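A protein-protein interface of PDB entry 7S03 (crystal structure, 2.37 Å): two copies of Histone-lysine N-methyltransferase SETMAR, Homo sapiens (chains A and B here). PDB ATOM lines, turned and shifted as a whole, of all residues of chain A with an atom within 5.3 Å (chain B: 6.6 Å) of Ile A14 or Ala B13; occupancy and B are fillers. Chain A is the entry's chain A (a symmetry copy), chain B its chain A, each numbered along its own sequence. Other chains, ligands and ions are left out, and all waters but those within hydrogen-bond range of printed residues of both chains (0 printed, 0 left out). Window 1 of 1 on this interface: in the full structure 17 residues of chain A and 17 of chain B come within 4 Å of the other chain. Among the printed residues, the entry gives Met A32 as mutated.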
ATOM      1  N   LEU A   6      25.101   4.862  22.907  1.00  0.00           N
ATOM      2  CA  LEU A   6      24.143   5.643  23.699  1.00  0.00           C
ATOM      3  C   LEU A   6      24.636   6.102  25.072  1.00  0.00           C
ATOM      4  O   LEU A   6      25.280   5.327  25.778  1.00  0.00           O
ATOM      5  CB  LEU A   6      22.806   4.890  23.846  1.00  0.00           C
ATOM      6  CG  LEU A   6      22.164   4.342  22.549  1.00  0.00           C
ATOM      7  CD1 LEU A   6      20.962   3.522  22.851  1.00  0.00           C
ATOM      8  CD2 LEU A   6      21.818   5.443  21.564  1.00  0.00           C
ATOM      9  N   GLN A  10      20.045   8.614  27.113  1.00  0.00           N
ATOM     10  CA  GLN A  10      19.398   7.974  25.977  1.00  0.00           C
ATOM     11  C   GLN A  10      18.878   6.604  26.389  1.00  0.00           C
ATOM     12  O   GLN A  10      17.750   6.259  26.060  1.00  0.00           O
ATOM     13  CB  GLN A  10      20.354   7.877  24.786  1.00  0.00           C
ATOM     14  CG  GLN A  10      20.557   9.218  24.090  1.00  0.00           C
ATOM     15  CD  GLN A  10      21.708   9.189  23.118  1.00  0.00           C
ATOM     16  OE1 GLN A  10      22.830   8.802  23.455  1.00  0.00           O
ATOM     17  NE2 GLN A  10      21.483   9.690  21.914  1.00  0.00           N
ATOM     18  N   ILE A  11      19.680   5.849  27.165  1.00  0.00           N
ATOM     19  CA  ILE A  11      19.310   4.555  27.712  1.00  0.00           C
ATOM     20  C   ILE A  11      18.069   4.731  28.595  1.00  0.00           C
ATOM     21  O   ILE A  11      17.116   3.977  28.456  1.00  0.00           O
ATOM     22  CB  ILE A  11      20.497   3.922  28.509  1.00  0.00           C
ATOM     23  CG1 ILE A  11      21.694   3.528  27.594  1.00  0.00           C
ATOM     24  CG2 ILE A  11      20.015   2.702  29.342  1.00  0.00           C
ATOM     25  CD1 ILE A  11      21.442   2.267  26.523  1.00  0.00           C
ATOM     26  N   ARG A  12      18.088   5.715  29.510  1.00  0.00           N
ATOM     27  CA  ARG A  12      16.978   5.994  30.441  1.00  0.00           C
ATOM     28  C   ARG A  12      15.698   6.413  29.749  1.00  0.00           C
ATOM     29  O   ARG A  12      14.630   6.124  30.259  1.00  0.00           O
ATOM     30  CB  ARG A  12      17.381   7.024  31.499  1.00  0.00           C
ATOM     31  CG  ARG A  12      18.410   6.496  32.454  1.00  0.00           C
ATOM     32  CD  ARG A  12      19.039   7.651  33.202  1.00  0.00           C
ATOM     33  NE  ARG A  12      20.125   7.186  34.066  1.00  0.00           N
ATOM     34  CZ  ARG A  12      20.781   7.944  34.937  1.00  0.00           C
ATOM     35  NH1 ARG A  12      20.448   9.214  35.104  1.00  0.00           N
ATOM     36  NH2 ARG A  12      21.744   7.426  35.679  1.00  0.00           N
ATOM     37  N   ALA A  13      15.796   7.100  28.591  1.00  0.00           N
ATOM     38  CA  ALA A  13      14.647   7.530  27.795  1.00  0.00           C
ATOM     39  C   ALA A  13      13.958   6.301  27.209  1.00  0.00           C
ATOM     40  O   ALA A  13      12.723   6.265  27.153  1.00  0.00           O
ATOM     41  CB  ALA A  13      15.110   8.451  26.700  1.00  0.00           C
ATOM     42  N   ILE A  14      14.761   5.259  26.830  1.00  0.00           N
ATOM     43  CA  ILE A  14      14.245   3.996  26.302  1.00  0.00           C
ATOM     44  C   ILE A  14      13.529   3.250  27.429  1.00  0.00           C
ATOM     45  O   ILE A  14      12.489   2.657  27.192  1.00  0.00           O
ATOM     46  CB  ILE A  14      15.351   3.162  25.596  1.00  0.00           C
ATOM     47  CG1 ILE A  14      15.886   3.920  24.355  1.00  0.00           C
ATOM     48  CG2 ILE A  14      14.832   1.738  25.230  1.00  0.00           C
ATOM     49  CD1 ILE A  14      17.207   3.358  23.709  1.00  0.00           C
ATOM     50  N   PHE A  15      14.062   3.307  28.663  1.00  0.00           N
ATOM     51  CA  PHE A  15      13.409   2.700  29.828  1.00  0.00           C
ATOM     52  C   PHE A  15      12.034   3.349  29.987  1.00  0.00           C
ATOM     53  O   PHE A  15      11.033   2.643  30.126  1.00  0.00           O
ATOM     54  CB  PHE A  15      14.218   2.977  31.110  1.00  0.00           C
ATOM     55  CG  PHE A  15      15.495   2.205  31.334  1.00  0.00           C
ATOM     56  CD1 PHE A  15      15.981   1.331  30.370  1.00  0.00           C
ATOM     57  CD2 PHE A  15      16.224   2.365  32.502  1.00  0.00           C
ATOM     58  CE1 PHE A  15      17.173   0.620  30.581  1.00  0.00           C
ATOM     59  CE2 PHE A  15      17.410   1.657  32.712  1.00  0.00           C
ATOM     60  CZ  PHE A  15      17.874   0.779  31.755  1.00  0.00           C
ATOM     61  N   LEU A  16      11.990   4.704  29.972  1.00  0.00           N
ATOM     62  CA  LEU A  16      10.749   5.463  30.138  1.00  0.00           C
ATOM     63  C   LEU A  16       9.743   5.119  29.076  1.00  0.00           C
ATOM     64  O   LEU A  16       8.605   4.849  29.435  1.00  0.00           O
ATOM     65  CB  LEU A  16      11.003   6.974  30.244  1.00  0.00           C
ATOM     66  CG  LEU A  16       9.779   7.839  30.578  1.00  0.00           C
ATOM     67  CD1 LEU A  16       9.178   7.473  31.930  1.00  0.00           C
ATOM     68  CD2 LEU A  16      10.114   9.334  30.488  1.00  0.00           C
ATOM     69  N   PHE A  17      10.168   5.038  27.789  1.00  0.00           N
ATOM     70  CA  PHE A  17       9.328   4.636  26.655  1.00  0.00           C
ATOM     71  C   PHE A  17       8.679   3.277  26.912  1.00  0.00           C
ATOM     72  O   PHE A  17       7.466   3.140  26.758  1.00  0.00           O
ATOM     73  CB  PHE A  17      10.129   4.589  25.328  1.00  0.00           C
ATOM     74  CG  PHE A  17       9.401   3.998  24.132  1.00  0.00           C
ATOM     75  CD1 PHE A  17       8.268   4.616  23.607  1.00  0.00           C
ATOM     76  CD2 PHE A  17       9.852   2.832  23.530  1.00  0.00           C
ATOM     77  CE1 PHE A  17       7.599   4.080  22.501  1.00  0.00           C
ATOM     78  CE2 PHE A  17       9.178   2.288  22.430  1.00  0.00           C
ATOM     79  CZ  PHE A  17       8.067   2.933  21.908  1.00  0.00           C
ATOM     80  N   GLU A  18       9.496   2.292  27.316  1.00  0.00           N
ATOM     81  CA  GLU A  18       9.103   0.925  27.606  1.00  0.00           C
ATOM     82  C   GLU A  18       8.150   0.820  28.789  1.00  0.00           C
ATOM     83  O   GLU A  18       7.156   0.090  28.715  1.00  0.00           O
ATOM     84  CB  GLU A  18      10.333   0.057  27.774  1.00  0.00           C
ATOM     85  CG  GLU A  18      10.996  -0.288  26.454  1.00  0.00           C
ATOM     86  CD  GLU A  18      10.385  -1.462  25.714  1.00  0.00           C
ATOM     87  OE1 GLU A  18      10.666  -2.617  26.104  1.00  0.00           O
ATOM     88  OE2 GLU A  18       9.634  -1.229  24.741  1.00  0.00           O
ATOM     89  N   PHE A  19       8.422   1.589  29.863  1.00  0.00           N
ATOM     90  CA  PHE A  19       7.543   1.671  31.037  1.00  0.00           C
ATOM     91  C   PHE A  19       6.171   2.204  30.600  1.00  0.00           C
ATOM     92  O   PHE A  19       5.155   1.657  31.008  1.00  0.00           O
ATOM     93  CB  PHE A  19       8.165   2.581  32.133  1.00  0.00           C
ATOM     94  CG  PHE A  19       7.190   2.920  33.236  1.00  0.00           C
ATOM     95  CD1 PHE A  19       6.921   2.007  34.251  1.00  0.00           C
ATOM     96  CD2 PHE A  19       6.481   4.124  33.217  1.00  0.00           C
ATOM     97  CE1 PHE A  19       5.969   2.293  35.230  1.00  0.00           C
ATOM     98  CE2 PHE A  19       5.519   4.407  34.199  1.00  0.00           C
ATOM     99  CZ  PHE A  19       5.271   3.491  35.198  1.00  0.00           C
ATOM    100  N   THR A  28      11.466  -5.533  29.298  1.00  0.00           N
ATOM    101  CA  THR A  28      12.240  -4.411  28.753  1.00  0.00           C
ATOM    102  C   THR A  28      13.726  -4.778  28.646  1.00  0.00           C
ATOM    103  O   THR A  28      14.354  -4.466  27.632  1.00  0.00           O
ATOM    104  CB  THR A  28      11.973  -3.171  29.622  1.00  0.00           C
ATOM    105  OG1 THR A  28      10.623  -2.793  29.403  1.00  0.00           O
ATOM    106  CG2 THR A  28      12.904  -1.985  29.319  1.00  0.00           C
ATOM    107  N   MET A  32      15.982  -4.883  25.241  1.00  0.00           N
ATOM    108  CA  MET A  32      17.185  -4.065  25.078  1.00  0.00           C
ATOM    109  C   MET A  32      18.429  -4.861  24.775  1.00  0.00           C
ATOM    110  O   MET A  32      19.213  -4.431  23.921  1.00  0.00           O
ATOM    111  CB  MET A  32      17.345  -3.171  26.272  1.00  0.00           C
ATOM    112  CG  MET A  32      16.160  -2.264  26.327  1.00  0.00           C
ATOM    113  SD  MET A  32      16.274  -0.884  27.562  1.00  0.00           S
ATOM    114  CE  MET A  32      17.788   0.088  26.692  1.00  0.00           C
ATOM    115  N   PHE A  36      20.150  -4.261  21.104  1.00  0.00           N
ATOM    116  CA  PHE A  36      21.487  -3.657  21.110  1.00  0.00           C
ATOM    117  C   PHE A  36      22.620  -4.623  21.399  1.00  0.00           C
ATOM    118  O   PHE A  36      23.766  -4.268  21.154  1.00  0.00           O
ATOM    119  CB  PHE A  36      21.551  -2.450  22.072  1.00  0.00           C
ATOM    120  CG  PHE A  36      20.651  -1.298  21.695  1.00  0.00           C
ATOM    121  CD1 PHE A  36      20.966  -0.466  20.621  1.00  0.00           C
ATOM    122  CD2 PHE A  36      19.489  -1.035  22.416  1.00  0.00           C
ATOM    123  CE1 PHE A  36      20.128   0.603  20.270  1.00  0.00           C
ATOM    124  CE2 PHE A  36      18.663   0.036  22.072  1.00  0.00           C
ATOM    125  CZ  PHE A  36      18.999   0.858  21.008  1.00  0.00           C
ATOM    126  N   LYS B   8      16.216  15.900  21.627  1.00  0.00           N
ATOM    127  CA  LYS B   8      16.141  15.289  20.285  1.00  0.00           C
ATOM    128  C   LYS B   8      16.935  13.979  20.291  1.00  0.00           C
ATOM    129  O   LYS B   8      16.482  13.006  19.733  1.00  0.00           O
ATOM    130  CB  LYS B   8      16.670  16.247  19.189  1.00  0.00           C
ATOM    131  CG  LYS B   8      15.577  17.137  18.606  1.00  0.00           C
ATOM    132  CD  LYS B   8      15.994  17.853  17.326  1.00  0.00           C
ATOM    133  CE  LYS B   8      14.809  18.545  16.689  1.00  0.00           C
ATOM    134  NZ  LYS B   8      15.207  19.424  15.558  1.00  0.00           N
ATOM    135  N   LYS B   9      18.058  13.940  21.014  1.00  0.00           N
ATOM    136  CA  LYS B   9      18.946  12.783  21.190  1.00  0.00           C
ATOM    137  C   LYS B   9      18.277  11.621  21.896  1.00  0.00           C
ATOM    138  O   LYS B   9      18.609  10.475  21.602  1.00  0.00           O
ATOM    139  CB  LYS B   9      20.233  13.179  21.967  1.00  0.00           C
ATOM    140  CG  LYS B   9      21.185  14.132  21.230  1.00  0.00           C
ATOM    141  CD  LYS B   9      21.665  13.642  19.850  1.00  0.00           C
ATOM    142  CE  LYS B   9      22.358  14.752  19.080  1.00  0.00           C
ATOM    143  NZ  LYS B   9      21.427  15.829  18.611  1.00  0.00           N
ATOM    144  N   GLN B  10      17.379  11.906  22.851  1.00  0.00           N
ATOM    145  CA  GLN B  10      16.632  10.893  23.582  1.00  0.00           C
ATOM    146  C   GLN B  10      15.526  10.335  22.697  1.00  0.00           C
ATOM    147  O   GLN B  10      15.345   9.125  22.645  1.00  0.00           O
ATOM    148  CB  GLN B  10      16.073  11.460  24.889  1.00  0.00           C
ATOM    149  CG  GLN B  10      17.147  11.634  25.956  1.00  0.00           C
ATOM    150  CD  GLN B  10      16.666  12.458  27.123  1.00  0.00           C
ATOM    151  OE1 GLN B  10      16.155  13.569  26.964  1.00  0.00           O
ATOM    152  NE2 GLN B  10      16.906  11.975  28.332  1.00  0.00           N
ATOM    153  N   ILE B  11      14.831  11.215  21.952  1.00  0.00           N
ATOM    154  CA  ILE B  11      13.799  10.847  20.998  1.00  0.00           C
ATOM    155  C   ILE B  11      14.418   9.933  19.933  1.00  0.00           C
ATOM    156  O   ILE B  11      13.856   8.890  19.631  1.00  0.00           O
ATOM    157  CB  ILE B  11      13.149  12.116  20.356  1.00  0.00           C
ATOM    158  CG1 ILE B  11      12.324  12.952  21.379  1.00  0.00           C
ATOM    159  CG2 ILE B  11      12.277  11.730  19.130  1.00  0.00           C
ATOM    160  CD1 ILE B  11      10.923  12.252  21.970  1.00  0.00           C
ATOM    161  N   ARG B  12      15.565  10.332  19.358  1.00  0.00           N
ATOM    162  CA  ARG B  12      16.267   9.569  18.308  1.00  0.00           C
ATOM    163  C   ARG B  12      16.757   8.212  18.770  1.00  0.00           C
ATOM    164  O   ARG B  12      16.811   7.299  17.965  1.00  0.00           O
ATOM    165  CB  ARG B  12      17.415  10.379  17.701  1.00  0.00           C
ATOM    166  CG  ARG B  12      16.932  11.555  16.905  1.00  0.00           C
ATOM    167  CD  ARG B  12      18.083  12.511  16.675  1.00  0.00           C
ATOM    168  NE  ARG B  12      17.628  13.724  15.994  1.00  0.00           N
ATOM    169  CZ  ARG B  12      18.423  14.687  15.545  1.00  0.00           C
ATOM    170  NH1 ARG B  12      19.736  14.581  15.664  1.00  0.00           N
ATOM    171  NH2 ARG B  12      17.913  15.743  14.935  1.00  0.00           N
ATOM    172  N   ALA B  13      17.121   8.074  20.062  1.00  0.00           N
ATOM    173  CA  ALA B  13      17.572   6.816  20.655  1.00  0.00           C
ATOM    174  C   ALA B  13      16.401   5.838  20.700  1.00  0.00           C
ATOM    175  O   ALA B  13      16.597   4.642  20.454  1.00  0.00           O
ATOM    176  CB  ALA B  13      18.102   7.072  22.039  1.00  0.00           C
ATOM    177  N   ILE B  14      15.162   6.363  20.953  1.00  0.00           N
ATOM    178  CA  ILE B  14      13.937   5.562  20.974  1.00  0.00           C
ATOM    179  C   ILE B  14      13.632   5.095  19.550  1.00  0.00           C
ATOM    180  O   ILE B  14      13.217   3.963  19.364  1.00  0.00           O
ATOM    181  CB  ILE B  14      12.760   6.311  21.660  1.00  0.00           C
ATOM    182  CG1 ILE B  14      13.087   6.575  23.152  1.00  0.00           C
ATOM    183  CG2 ILE B  14      11.422   5.531  21.486  1.00  0.00           C
ATOM    184  CD1 ILE B  14      12.140   7.582  23.906  1.00  0.00           C
ATOM    185  N   PHE B  15      13.869   5.952  18.540  1.00  0.00           N
ATOM    186  CA  PHE B  15      13.692   5.575  17.134  1.00  0.00           C
ATOM    187  C   PHE B  15      14.618   4.393  16.844  1.00  0.00           C
ATOM    188  O   PHE B  15      14.175   3.387  16.285  1.00  0.00           O
ATOM    189  CB  PHE B  15      14.096   6.736  16.204  1.00  0.00           C
ATOM    190  CG  PHE B  15      13.161   7.914  16.080  1.00  0.00           C
ATOM    191  CD1 PHE B  15      12.007   7.996  16.849  1.00  0.00           C
ATOM    192  CD2 PHE B  15      13.442   8.952  15.206  1.00  0.00           C
ATOM    193  CE1 PHE B  15      11.145   9.098  16.734  1.00  0.00           C
ATOM    194  CE2 PHE B  15      12.583  10.048  15.091  1.00  0.00           C
ATOM    195  CZ  PHE B  15      11.432  10.111  15.848  1.00  0.00           C
ATOM    196  N   LEU B  16      15.913   4.523  17.223  1.00  0.00           N
ATOM    197  CA  LEU B  16      16.920   3.486  16.989  1.00  0.00           C
ATOM    198  C   LEU B  16      16.542   2.189  17.648  1.00  0.00           C
ATOM    199  O   LEU B  16      16.594   1.170  16.974  1.00  0.00           O
ATOM    200  CB  LEU B  16      18.333   3.952  17.368  1.00  0.00           C
ATOM    201  CG  LEU B  16      19.476   2.991  17.011  1.00  0.00           C
ATOM    202  CD1 LEU B  16      19.562   2.746  15.509  1.00  0.00           C
ATOM    203  CD2 LEU B  16      20.812   3.479  17.587  1.00  0.00           C
ATOM    204  N   PHE B  17      16.082   2.227  18.925  1.00  0.00           N
ATOM    205  CA  PHE B  17      15.600   1.060  19.675  1.00  0.00           C
ATOM    206  C   PHE B  17      14.494   0.338  18.906  1.00  0.00           C
ATOM    207  O   PHE B  17      14.567  -0.877  18.729  1.00  0.00           O
ATOM    208  CB  PHE B  17      15.087   1.450  21.085  1.00  0.00           C
ATOM    209  CG  PHE B  17      14.388   0.349  21.866  1.00  0.00           C
ATOM    210  CD1 PHE B  17      15.078  -0.796  22.262  1.00  0.00           C
ATOM    211  CD2 PHE B  17      13.049   0.461  22.210  1.00  0.00           C
ATOM    212  CE1 PHE B  17      14.442  -1.808  22.989  1.00  0.00           C
ATOM    213  CE2 PHE B  17      12.407  -0.557  22.927  1.00  0.00           C
ATOM    214  CZ  PHE B  17      13.119  -1.675  23.333  1.00  0.00           C
ATOM    215  N   GLU B  18      13.489   1.100  18.448  1.00  0.00           N
ATOM    216  CA  GLU B  18      12.333   0.629  17.707  1.00  0.00           C
ATOM    217  C   GLU B  18      12.697   0.036  16.354  1.00  0.00           C
ATOM    218  O   GLU B  18      12.181  -1.025  15.988  1.00  0.00           O
ATOM    219  CB  GLU B  18      11.302   1.735  17.597  1.00  0.00           C
ATOM    220  CG  GLU B  18      10.536   1.956  18.888  1.00  0.00           C
ATOM    221  CD  GLU B  18       9.365   1.017  19.109  1.00  0.00           C
ATOM    222  OE1 GLU B  18       8.301   1.244  18.492  1.00  0.00           O
ATOM    223  OE2 GLU B  18       9.508   0.063  19.905  1.00  0.00           O
ATOM    224  N   PHE B  53      19.163   4.581   9.189  1.00  0.00           N
ATOM    225  CA  PHE B  53      19.520   3.405   9.986  1.00  0.00           C
ATOM    226  C   PHE B  53      19.677   2.172   9.108  1.00  0.00           C
ATOM    227  O   PHE B  53      20.607   1.392   9.314  1.00  0.00           O
ATOM    228  CB  PHE B  53      18.452   3.142  11.068  1.00  0.00           C
ATOM    229  CG  PHE B  53      18.200   4.240  12.091  1.00  0.00           C
ATOM    230  CD1 PHE B  53      19.180   5.190  12.384  1.00  0.00           C
ATOM    231  CD2 PHE B  53      17.005   4.289  12.801  1.00  0.00           C
ATOM    232  CE1 PHE B  53      18.957   6.167  13.346  1.00  0.00           C
ATOM    233  CE2 PHE B  53      16.784   5.269  13.756  1.00  0.00           C
ATOM    234  CZ  PHE B  53      17.764   6.190  14.037  1.00  0.00           C
ATOM    235  N   LEU B  60      23.139   9.461  15.719  1.00  0.00           N
ATOM    236  CA  LEU B  60      21.915  10.193  16.049  1.00  0.00           C
ATOM    237  C   LEU B  60      22.162  11.703  16.048  1.00  0.00           C
ATOM    238  O   LEU B  60      21.325  12.475  16.509  1.00  0.00           O
ATOM    239  CB  LEU B  60      21.271   9.667  17.359  1.00  0.00           C
ATOM    240  CG  LEU B  60      21.098   8.118  17.453  1.00  0.00           C
ATOM    241  CD1 LEU B  60      20.670   7.697  18.812  1.00  0.00           C
ATOM    242  CD2 LEU B  60      20.109   7.600  16.465  1.00  0.00           C
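O of Leu B60 lies within hydrogen-bond range of NH1 of Arg B12, at 2.8 Å.
The side-chain carboxylate of Glu A18 sits close to the side-chain hydroxyl of Thr A28, at 3.3 Å.
Among the printed residues, pairs that only touch across the chains: Leu A6 with Leu B60, Gln A10 with Ala B13, Gln A10 with Leu B60, Ala A13 with Gln B10, Ala A13 with Ile B14, Ile A14 with Ala B13, Ile A14 with Phe B17, Phe A17 with Ile B14, Phe A17 with Glu B18, Glu A18 with Phe B17, Met A32 with Phe B17, Phe A36 with Leu B16 and Phe A36 with Phe B17.
The backbone carbonyl oxygen of Lys B9 lies within hydrogen-bond range of the side-chain amide nitrogen of Gln A10, at 3.0 Å.
Gln A10 touches Ala B13, and with the chains exchanged Ala A13 touches Gln B10.
Ala A13 touches Ile B14, and with the chains exchanged Ile A14 touches Ala B13.
Ile A14 touches Phe B17, and with the chains exchanged Phe A17 touches Ile B14.
Phe A17 touches Glu B18, and with the chains exchanged Glu A18 touches Phe B17.
Positions printed for both chains: 10, 11, 12, 13, 14, 15, 16, 17 and 18.
Of the 14 printed residues of chain A, 8 touch a printed residue of chain B.
Printed residues of chain A that touch a printed residue of chain B: Leu A6, Gln A10, Ala A13, Ile A14, Phe A17, Glu A18, Met A32 and Phe A36.
Among the printed residues, 14 pairs touch across the chains.
Among the printed residues, no Asp or Glu carboxylate lies within 4 Å of a Lys or Arg side-chain nitrogen of the other chain.
Ile A14 touches just these residues of chain B: Ala B13 and Phe B17.
Ala B13 touches just these residues of chain A: Gln A10 (3.6 Å) and Ile A14 (3.6 Å).
Of the printed residues of chain A, Lys B9 touches Gln A10 (3.0 Å).
Of the printed residues of chain A, Glu B18 touches Phe A17 (3.4 Å).
Printed residues of chain B within 4 Å of Phe A17: Ile B14 (3.7 Å) and Glu B18 (3.4 Å).
Printed residues of chain A within 4 Å of Gln B10: Ala A13.
Of the printed residues of chain B, Phe A36 touches Leu B16 and Phe B17.
The nearest residue of chain B that does not touch Ile A14 is Ile B14 (4.04 Å).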
